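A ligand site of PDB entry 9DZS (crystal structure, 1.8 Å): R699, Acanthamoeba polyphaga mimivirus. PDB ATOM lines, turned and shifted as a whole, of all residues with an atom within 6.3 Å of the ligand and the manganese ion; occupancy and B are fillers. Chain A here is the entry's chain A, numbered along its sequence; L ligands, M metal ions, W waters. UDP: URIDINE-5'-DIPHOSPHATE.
Water W4 lies within hydrogen-bond range of the side-chain hydroxyl (OH) of Tyr 88 (2.7 Å), the side-chain hydroxyl (OG) of Ser 21 (3.0 Å) and an oxygen (O4) of the ligand (3.0 Å).
The side-chain amino group of Lys 225 lies within salt-bridge range of an oxygen (O1B) of the ligand (2.8 Å). O of Ile 20 sits at hydrogen-bond distance from N3 of the ligand, at 2.7 Å. N3 of the ligand lies within hydrogen-bond range of OH of Tyr 88. N of Ile 20 lies within hydrogen-bond range of O2 of the ligand (2.8 Å). N of Thr 87 sits at hydrogen-bond distance from O2' of the ligand (3.0 Å). An oxygen (O3') of the ligand lies within hydrogen-bond range of the backbone NH (N) of Tyr 88 (3.2 Å). The backbone carbonyl oxygen of Ile 18 sits at hydrogen-bond distance from an oxygen (O2') of the ligand, at 2.7 Å. The backbone NH (N) of Gly 222 is in hydrogen-bond range of an oxygen (O1B) of the ligand (2.8 Å).
Within 4 Å of the manganese ion: Asp 86, Asp 89 and His 219.
Residues that only touch the ligand: Trp 51, Leu 56, Lys 65, Gly 19 and Asn 221. Hydrophobic or aromatic side chains that line the ligand: Ile 18, Ile 20, Trp 51, Leu 56, Tyr 88 and His 219. 14 residues have an atom within 4 Å of the ligand: Ile 18, Gly 19, Ile 20, Trp 51, Leu 56, Lys 65, Asp 86, Thr 87, Tyr 88, Asp 89, His 219, Asn 221, Gly 222 and Lys 225.
The backbone carbonyl oxygen (O) of Ile 18 is in hydrogen-bond range of the side-chain hydroxyl (OG1) of Thr 87, 2.7 Å away. N of Ile 18 is in hydrogen-bond range of O of Cys 85, at 2.9 Å. The backbone NH (N) of Lys 225 sits at hydrogen-bond distance from the backbone carbonyl oxygen (O) of Gly 220, at 3.1 Å. The backbone carbonyl oxygen (O) of Val 45 is in hydrogen-bond range of the backbone NH (N) of Gly 19, 2.9 Å away. The backbone NH (N) of Asp 86 is in hydrogen-bond range of the backbone carbonyl oxygen (O) of Gly 143 (2.9 Å). The side-chain amide oxygen (OD1) of Asn 221 sits close to the backbone carbonyl oxygen (O) of His 219 (3.4 Å). The backbone carbonyl oxygen (O) of Gly 54 is in hydrogen-bond range of the indole nitrogen (NE1) of Trp 51. OD2 of Asp 89 lies close to NZ of Lys 225, at 2.8 Å.
The manganese ion is bound by O2B of the ligand (2.1 Å), OD2 of Asp 86 (2.2 Å), O2A of the ligand (2.2 Å), OD2 of Asp 89 (2.2 Å), NE2 of His 219 (2.2 Å) and OD1 of Asp 89 (2.4 Å). The manganese ion has six donor atoms within binding distance.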
ATOM      1  N   GLY A  17      21.269  11.103  16.790  1.00  0.00           N
ATOM      2  CA  GLY A  17      22.257  10.121  16.346  1.00  0.00           C
ATOM      3  C   GLY A  17      22.029   9.795  14.884  1.00  0.00           C
ATOM      4  O   GLY A  17      20.887   9.492  14.467  1.00  0.00           O
ATOM      5  N   ILE A  18      23.117   9.806  14.108  1.00  0.00           N
ATOM      6  CA  ILE A  18      23.026   9.486  12.690  1.00  0.00           C
ATOM      7  C   ILE A  18      22.952   7.967  12.527  1.00  0.00           C
ATOM      8  O   ILE A  18      23.863   7.244  12.931  1.00  0.00           O
ATOM      9  CB  ILE A  18      24.220  10.070  11.915  1.00  0.00           C
ATOM     10  CG1 ILE A  18      24.484  11.595  12.195  1.00  0.00           C
ATOM     11  CG2 ILE A  18      24.064   9.746  10.418  1.00  0.00           C
ATOM     12  CD1 ILE A  18      23.291  12.524  12.008  1.00  0.00           C
ATOM     13  N   GLY A  19      21.845   7.493  11.963  1.00  0.00           N
ATOM     14  CA  GLY A  19      21.655   6.067  11.702  1.00  0.00           C
ATOM     15  C   GLY A  19      20.898   5.863  10.392  1.00  0.00           C
ATOM     16  O   GLY A  19      19.713   5.516  10.383  1.00  0.00           O
ATOM     17  N   ILE A  20      21.623   6.121   9.289  1.00  0.00           N
ATOM     18  CA  ILE A  20      21.091   6.034   7.942  1.00  0.00           C
ATOM     19  C   ILE A  20      21.257   4.586   7.482  1.00  0.00           C
ATOM     20  O   ILE A  20      22.368   4.154   7.163  1.00  0.00           O
ATOM     21  CB  ILE A  20      21.846   6.984   6.995  1.00  0.00           C
ATOM     22  CG1 ILE A  20      21.781   8.461   7.483  1.00  0.00           C
ATOM     23  CG2 ILE A  20      21.302   6.835   5.567  1.00  0.00           C
ATOM     24  CD1 ILE A  20      22.908   9.357   6.930  1.00  0.00           C
ATOM     25  N   SER A  21      20.117   3.881   7.398  1.00  0.00           N
ATOM     26  CA  SER A  21      20.086   2.478   7.031  1.00  0.00           C
ATOM     27  C   SER A  21      18.613   2.088   6.841  1.00  0.00           C
ATOM     28  O   SER A  21      17.744   2.570   7.566  1.00  0.00           O
ATOM     29  CB  SER A  21      20.666   1.630   8.143  1.00  0.00           C
ATOM     30  OG  SER A  21      20.922   0.314   7.639  1.00  0.00           O
ATOM     31  N   VAL A  45      18.608   9.924  13.165  1.00  0.00           N
ATOM     32  CA  VAL A  45      18.526  10.677  11.920  1.00  0.00           C
ATOM     33  C   VAL A  45      18.748   9.728  10.749  1.00  0.00           C
ATOM     34  O   VAL A  45      19.721   8.996  10.712  1.00  0.00           O
ATOM     35  CB  VAL A  45      19.605  11.772  11.932  1.00  0.00           C
ATOM     36  CG1 VAL A  45      19.765  12.417  10.543  1.00  0.00           C
ATOM     37  CG2 VAL A  45      19.285  12.838  12.991  1.00  0.00           C
ATOM     38  N   TRP A  51      22.014   4.239   2.783  1.00  0.00           N
ATOM     39  CA  TRP A  51      23.261   4.954   2.921  1.00  0.00           C
ATOM     40  C   TRP A  51      23.895   5.229   1.550  1.00  0.00           C
ATOM     41  O   TRP A  51      24.026   4.325   0.732  1.00  0.00           O
ATOM     42  CB  TRP A  51      24.224   4.157   3.813  1.00  0.00           C
ATOM     43  CG  TRP A  51      25.639   4.663   3.872  1.00  0.00           C
ATOM     44  CD1 TRP A  51      26.703   4.095   3.244  1.00  0.00           C
ATOM     45  CD2 TRP A  51      26.165   5.765   4.650  1.00  0.00           C
ATOM     46  NE1 TRP A  51      27.853   4.793   3.526  1.00  0.00           N
ATOM     47  CE2 TRP A  51      27.555   5.799   4.415  1.00  0.00           C
ATOM     48  CE3 TRP A  51      25.611   6.705   5.519  1.00  0.00           C
ATOM     49  CZ2 TRP A  51      28.387   6.746   5.020  1.00  0.00           C
ATOM     50  CZ3 TRP A  51      26.442   7.614   6.143  1.00  0.00           C
ATOM     51  CH2 TRP A  51      27.816   7.640   5.894  1.00  0.00           C
ATOM     52  N   GLY A  54      29.323   6.885   1.121  1.00  0.00           N
ATOM     53  CA  GLY A  54      30.587   6.389   0.577  1.00  0.00           C
ATOM     54  C   GLY A  54      31.111   5.211   1.398  1.00  0.00           C
ATOM     55  O   GLY A  54      30.648   4.987   2.506  1.00  0.00           O
ATOM     56  N   LEU A  56      33.369   4.306   3.708  1.00  0.00           N
ATOM     57  CA  LEU A  56      34.171   5.069   4.654  1.00  0.00           C
ATOM     58  C   LEU A  56      35.499   4.366   4.960  1.00  0.00           C
ATOM     59  O   LEU A  56      36.517   5.018   5.188  1.00  0.00           O
ATOM     60  CB  LEU A  56      33.377   5.413   5.911  1.00  0.00           C
ATOM     61  CG  LEU A  56      32.253   6.451   5.767  1.00  0.00           C
ATOM     62  CD1 LEU A  56      31.689   6.801   7.123  1.00  0.00           C
ATOM     63  CD2 LEU A  56      32.681   7.716   5.034  1.00  0.00           C
ATOM     64  N   LYS A  65      25.576  12.489   5.889  1.00  0.00           N
ATOM     65  CA  LYS A  65      25.210  12.670   7.287  1.00  0.00           C
ATOM     66  C   LYS A  65      24.745  14.110   7.541  1.00  0.00           C
ATOM     67  O   LYS A  65      23.786  14.361   8.269  1.00  0.00           O
ATOM     68  CB  LYS A  65      26.387  12.350   8.227  1.00  0.00           C
ATOM     69  CG  LYS A  65      26.925  10.917   8.115  1.00  0.00           C
ATOM     70  CD  LYS A  65      27.885  10.611   9.270  1.00  0.00           C
ATOM     71  CE  LYS A  65      29.147  11.383   9.253  1.00  0.00           C
ATOM     72  NZ  LYS A  65      29.844  11.277  10.537  1.00  0.00           N
ATOM     73  N   CYS A  85      25.737  12.992  16.796  1.00  0.00           N
ATOM     74  CA  CYS A  85      26.787  11.998  16.993  1.00  0.00           C
ATOM     75  C   CYS A  85      26.581  10.787  16.077  1.00  0.00           C
ATOM     76  O   CYS A  85      25.459  10.430  15.727  1.00  0.00           O
ATOM     77  CB  CYS A  85      26.884  11.570  18.468  1.00  0.00           C
ATOM     78  SG  CYS A  85      25.353  10.832  19.097  1.00  0.00           S
ATOM     79  N   ASP A  86      27.708  10.128  15.822  1.00  0.00           N
ATOM     80  CA  ASP A  86      27.730   8.783  15.268  1.00  0.00           C
ATOM     81  C   ASP A  86      26.936   7.857  16.170  1.00  0.00           C
ATOM     82  O   ASP A  86      26.829   8.122  17.377  1.00  0.00           O
ATOM     83  CB  ASP A  86      29.164   8.266  15.211  1.00  0.00           C
ATOM     84  CG  ASP A  86      30.033   8.839  14.104  1.00  0.00           C
ATOM     85  OD1 ASP A  86      29.588   9.794  13.412  1.00  0.00           O
ATOM     86  OD2 ASP A  86      31.188   8.379  13.972  1.00  0.00           O
ATOM     87  N   THR A  87      26.439   6.732  15.608  1.00  0.00           N
ATOM     88  CA  THR A  87      25.725   5.753  16.450  1.00  0.00           C
ATOM     89  C   THR A  87      26.313   4.346  16.306  1.00  0.00           C
ATOM     90  O   THR A  87      26.044   3.502  17.175  1.00  0.00           O
ATOM     91  CB  THR A  87      24.223   5.694  16.196  1.00  0.00           C
ATOM     92  OG1 THR A  87      24.059   5.280  14.837  1.00  0.00           O
ATOM     93  CG2 THR A  87      23.578   7.069  16.422  1.00  0.00           C
ATOM     94  N   TYR A  88      27.048   4.074  15.222  1.00  0.00           N
ATOM     95  CA  TYR A  88      27.403   2.677  14.995  1.00  0.00           C
ATOM     96  C   TYR A  88      28.437   2.192  16.004  1.00  0.00           C
ATOM     97  O   TYR A  88      28.481   0.984  16.345  1.00  0.00           O
ATOM     98  CB  TYR A  88      27.891   2.464  13.554  1.00  0.00           C
ATOM     99  CG  TYR A  88      26.747   2.392  12.546  1.00  0.00           C
ATOM    100  CD1 TYR A  88      25.469   2.897  12.849  1.00  0.00           C
ATOM    101  CD2 TYR A  88      26.954   1.815  11.297  1.00  0.00           C
ATOM    102  CE1 TYR A  88      24.441   2.854  11.902  1.00  0.00           C
ATOM    103  CE2 TYR A  88      25.927   1.741  10.363  1.00  0.00           C
ATOM    104  CZ  TYR A  88      24.681   2.272  10.672  1.00  0.00           C
ATOM    105  OH  TYR A  88      23.680   2.157   9.733  1.00  0.00           O
ATOM    106  N   ASP A  89      29.249   3.126  16.474  1.00  0.00           N
ATOM    107  CA  ASP A  89      30.442   2.863  17.274  1.00  0.00           C
ATOM    108  C   ASP A  89      30.522   3.838  18.452  1.00  0.00           C
ATOM    109  O   ASP A  89      31.600   4.289  18.841  1.00  0.00           O
ATOM    110  CB  ASP A  89      31.679   3.029  16.421  1.00  0.00           C
ATOM    111  CG  ASP A  89      31.894   4.407  15.787  1.00  0.00           C
ATOM    112  OD1 ASP A  89      30.963   5.222  15.817  1.00  0.00           O
ATOM    113  OD2 ASP A  89      33.000   4.649  15.307  1.00  0.00           O
ATOM    114  N   LEU A  90      29.367   4.192  19.013  1.00  0.00           N
ATOM    115  CA  LEU A  90      29.330   5.214  20.049  1.00  0.00           C
ATOM    116  C   LEU A  90      28.164   4.973  21.019  1.00  0.00           C
ATOM    117  O   LEU A  90      27.060   4.624  20.610  1.00  0.00           O
ATOM    118  CB  LEU A  90      29.195   6.579  19.334  1.00  0.00           C
ATOM    119  CG  LEU A  90      29.220   7.831  20.227  1.00  0.00           C
ATOM    120  CD1 LEU A  90      29.695   9.057  19.381  1.00  0.00           C
ATOM    121  CD2 LEU A  90      27.849   8.179  20.809  1.00  0.00           C
ATOM    122  N   TRP A 121      43.326  14.760  10.298  1.00  0.00           N
ATOM    123  CA  TRP A 121      42.964  14.080   9.064  1.00  0.00           C
ATOM    124  C   TRP A 121      41.647  14.630   8.535  1.00  0.00           C
ATOM    125  O   TRP A 121      40.857  15.164   9.304  1.00  0.00           O
ATOM    126  CB  TRP A 121      42.873  12.562   9.287  1.00  0.00           C
ATOM    127  CG  TRP A 121      41.662  12.173  10.097  1.00  0.00           C
ATOM    128  CD1 TRP A 121      41.577  12.199  11.459  1.00  0.00           C
ATOM    129  CD2 TRP A 121      40.377  11.745   9.616  1.00  0.00           C
ATOM    130  NE1 TRP A 121      40.328  11.810  11.866  1.00  0.00           N
ATOM    131  CE2 TRP A 121      39.574  11.494  10.763  1.00  0.00           C
ATOM    132  CE3 TRP A 121      39.820  11.514   8.349  1.00  0.00           C
ATOM    133  CZ2 TRP A 121      38.253  11.043  10.683  1.00  0.00           C
ATOM    134  CZ3 TRP A 121      38.522  11.039   8.265  1.00  0.00           C
ATOM    135  CH2 TRP A 121      37.751  10.813   9.418  1.00  0.00           C
ATOM    136  N   ASN A 141      37.531  15.929  15.803  1.00  0.00           N
ATOM    137  CA  ASN A 141      36.896  14.705  15.320  1.00  0.00           C
ATOM    138  C   ASN A 141      35.404  15.007  15.143  1.00  0.00           C
ATOM    139  O   ASN A 141      34.751  15.514  16.054  1.00  0.00           O
ATOM    140  CB  ASN A 141      37.120  13.521  16.271  1.00  0.00           C
ATOM    141  CG  ASN A 141      36.349  12.321  15.746  1.00  0.00           C
ATOM    142  OD1 ASN A 141      35.147  12.205  16.008  1.00  0.00           O
ATOM    143  ND2 ASN A 141      37.003  11.430  15.013  1.00  0.00           N
ATOM    144  N   GLY A 143      32.773  13.147  14.687  1.00  0.00           N
ATOM    145  CA  GLY A 143      31.899  12.055  15.110  1.00  0.00           C
ATOM    146  C   GLY A 143      30.981  12.403  16.309  1.00  0.00           C
ATOM    147  O   GLY A 143      30.021  11.689  16.585  1.00  0.00           O
ATOM    148  N   HIS A 219      33.297   6.993  22.076  1.00  0.00           N
ATOM    149  CA  HIS A 219      33.316   6.850  20.636  1.00  0.00           C
ATOM    150  C   HIS A 219      34.475   5.930  20.242  1.00  0.00           C
ATOM    151  O   HIS A 219      35.643   6.320  20.320  1.00  0.00           O
ATOM    152  CB  HIS A 219      33.400   8.235  19.972  1.00  0.00           C
ATOM    153  CG  HIS A 219      33.333   8.134  18.493  1.00  0.00           C
ATOM    154  ND1 HIS A 219      33.731   9.177  17.686  1.00  0.00           N
ATOM    155  CD2 HIS A 219      32.905   7.154  17.676  1.00  0.00           C
ATOM    156  CE1 HIS A 219      33.557   8.849  16.411  1.00  0.00           C
ATOM    157  NE2 HIS A 219      33.039   7.617  16.387  1.00  0.00           N
ATOM    158  N   GLY A 220      34.141   4.716  19.795  1.00  0.00           N
ATOM    159  CA  GLY A 220      35.177   3.785  19.313  1.00  0.00           C
ATOM    160  C   GLY A 220      35.516   4.079  17.852  1.00  0.00           C
ATOM    161  O   GLY A 220      35.233   3.270  16.973  1.00  0.00           O
ATOM    162  N   ASN A 221      36.082   5.274  17.592  1.00  0.00           N
ATOM    163  CA  ASN A 221      36.275   5.746  16.226  1.00  0.00           C
ATOM    164  C   ASN A 221      37.338   4.860  15.552  1.00  0.00           C
ATOM    165  O   ASN A 221      38.272   4.367  16.208  1.00  0.00           O
ATOM    166  CB  ASN A 221      36.656   7.231  16.179  1.00  0.00           C
ATOM    167  CG  ASN A 221      37.945   7.554  16.945  1.00  0.00           C
ATOM    168  OD1 ASN A 221      38.085   7.167  18.112  1.00  0.00           O
ATOM    169  ND2 ASN A 221      38.873   8.293  16.325  1.00  0.00           N
ATOM    170  N   GLY A 222      37.214   4.703  14.232  1.00  0.00           N
ATOM    171  CA  GLY A 222      38.158   3.865  13.487  1.00  0.00           C
ATOM    172  C   GLY A 222      38.240   2.455  14.083  1.00  0.00           C
ATOM    173  O   GLY A 222      37.226   1.853  14.441  1.00  0.00           O
ATOM    174  N   PRO A 223      39.452   1.878  14.180  1.00  0.00           N
ATOM    175  CA  PRO A 223      39.675   0.556  14.760  1.00  0.00           C
ATOM    176  C   PRO A 223      39.337   0.452  16.240  1.00  0.00           C
ATOM    177  O   PRO A 223      39.269  -0.656  16.768  1.00  0.00           O
ATOM    178  CB  PRO A 223      41.216   0.356  14.576  1.00  0.00           C
ATOM    179  CG  PRO A 223      41.578   1.297  13.440  1.00  0.00           C
ATOM    180  CD  PRO A 223      40.693   2.500  13.673  1.00  0.00           C
ATOM    181  N   LYS A 225      36.546   0.533  17.481  1.00  0.00           N
ATOM    182  CA  LYS A 225      35.322  -0.242  17.636  1.00  0.00           C
ATOM    183  C   LYS A 225      35.596  -1.467  18.516  1.00  0.00           C
ATOM    184  O   LYS A 225      34.766  -1.830  19.353  1.00  0.00           O
ATOM    185  CB  LYS A 225      34.715  -0.656  16.285  1.00  0.00           C
ATOM    186  CG  LYS A 225      34.200   0.563  15.494  1.00  0.00           C
ATOM    187  CD  LYS A 225      34.126   0.420  13.998  1.00  0.00           C
ATOM    188  CE  LYS A 225      33.742   1.760  13.364  1.00  0.00           C
ATOM    189  NZ  LYS A 225      34.614   2.884  13.810  1.00  0.00           N
HETATM  190  N1  UDP L   1      26.592   5.657   9.171  1.00  0.00           N
HETATM  191  C2  UDP L   1      25.259   5.449   8.914  1.00  0.00           C
HETATM  192  N3  UDP L   1      24.965   4.493   7.971  1.00  0.00           N
HETATM  193  C4  UDP L   1      25.880   3.658   7.336  1.00  0.00           C
HETATM  194  C5  UDP L   1      27.254   3.925   7.650  1.00  0.00           C
HETATM  195  C6  UDP L   1      27.552   4.871   8.570  1.00  0.00           C
HETATM  196  O2  UDP L   1      24.398   6.112   9.477  1.00  0.00           O
HETATM  197  O4  UDP L   1      25.483   2.809   6.531  1.00  0.00           O
HETATM  198  C1' UDP L   1      26.897   6.666  10.215  1.00  0.00           C
HETATM  199  C2' UDP L   1      26.951   6.036  11.633  1.00  0.00           C
HETATM  200  O2' UDP L   1      26.488   6.954  12.606  1.00  0.00           O
HETATM  201  C3' UDP L   1      28.463   5.841  11.808  1.00  0.00           C
HETATM  202  C4' UDP L   1      28.999   7.130  11.172  1.00  0.00           C
HETATM  203  O4' UDP L   1      28.185   7.213   9.976  1.00  0.00           O
HETATM  204  O3' UDP L   1      28.796   5.717  13.177  1.00  0.00           O
HETATM  205  C5' UDP L   1      30.460   7.230  10.777  1.00  0.00           C
HETATM  206  O5' UDP L   1      30.981   5.915  10.403  1.00  0.00           O
HETATM  207  PA  UDP L   1      32.043   5.259  11.393  1.00  0.00           P
HETATM  208  O1A UDP L   1      32.344   3.864  10.979  1.00  0.00           O
HETATM  209  O2A UDP L   1      31.609   5.482  12.801  1.00  0.00           O
HETATM  210  O3A UDP L   1      33.326   6.187  11.133  1.00  0.00           O
HETATM  211  PB  UDP L   1      34.595   6.432  12.075  1.00  0.00           P
HETATM  212  O1B UDP L   1      35.269   5.092  12.254  1.00  0.00           O
HETATM  213  O2B UDP L   1      34.111   7.095  13.348  1.00  0.00           O
HETATM  214  O3B UDP L   1      35.445   7.449  11.251  1.00  0.00           O
HETATM  215 MN    MN M   1      32.381   6.632  14.489  1.00  0.00          MN
HETATM  216  O   HOH W   1      36.102   3.405  10.391  1.00  0.00           O
HETATM  217  O   HOH W   2      30.597   1.946  11.329  1.00  0.00           O
HETATM  218  O   HOH W   3      33.962   2.595   9.247  1.00  0.00           O
HETATM  219  O   HOH W   4      23.918   0.472   7.679  1.00  0.00           O
HETATM  220  O   HOH W   5      23.289   1.370   5.201  1.00  0.00           O
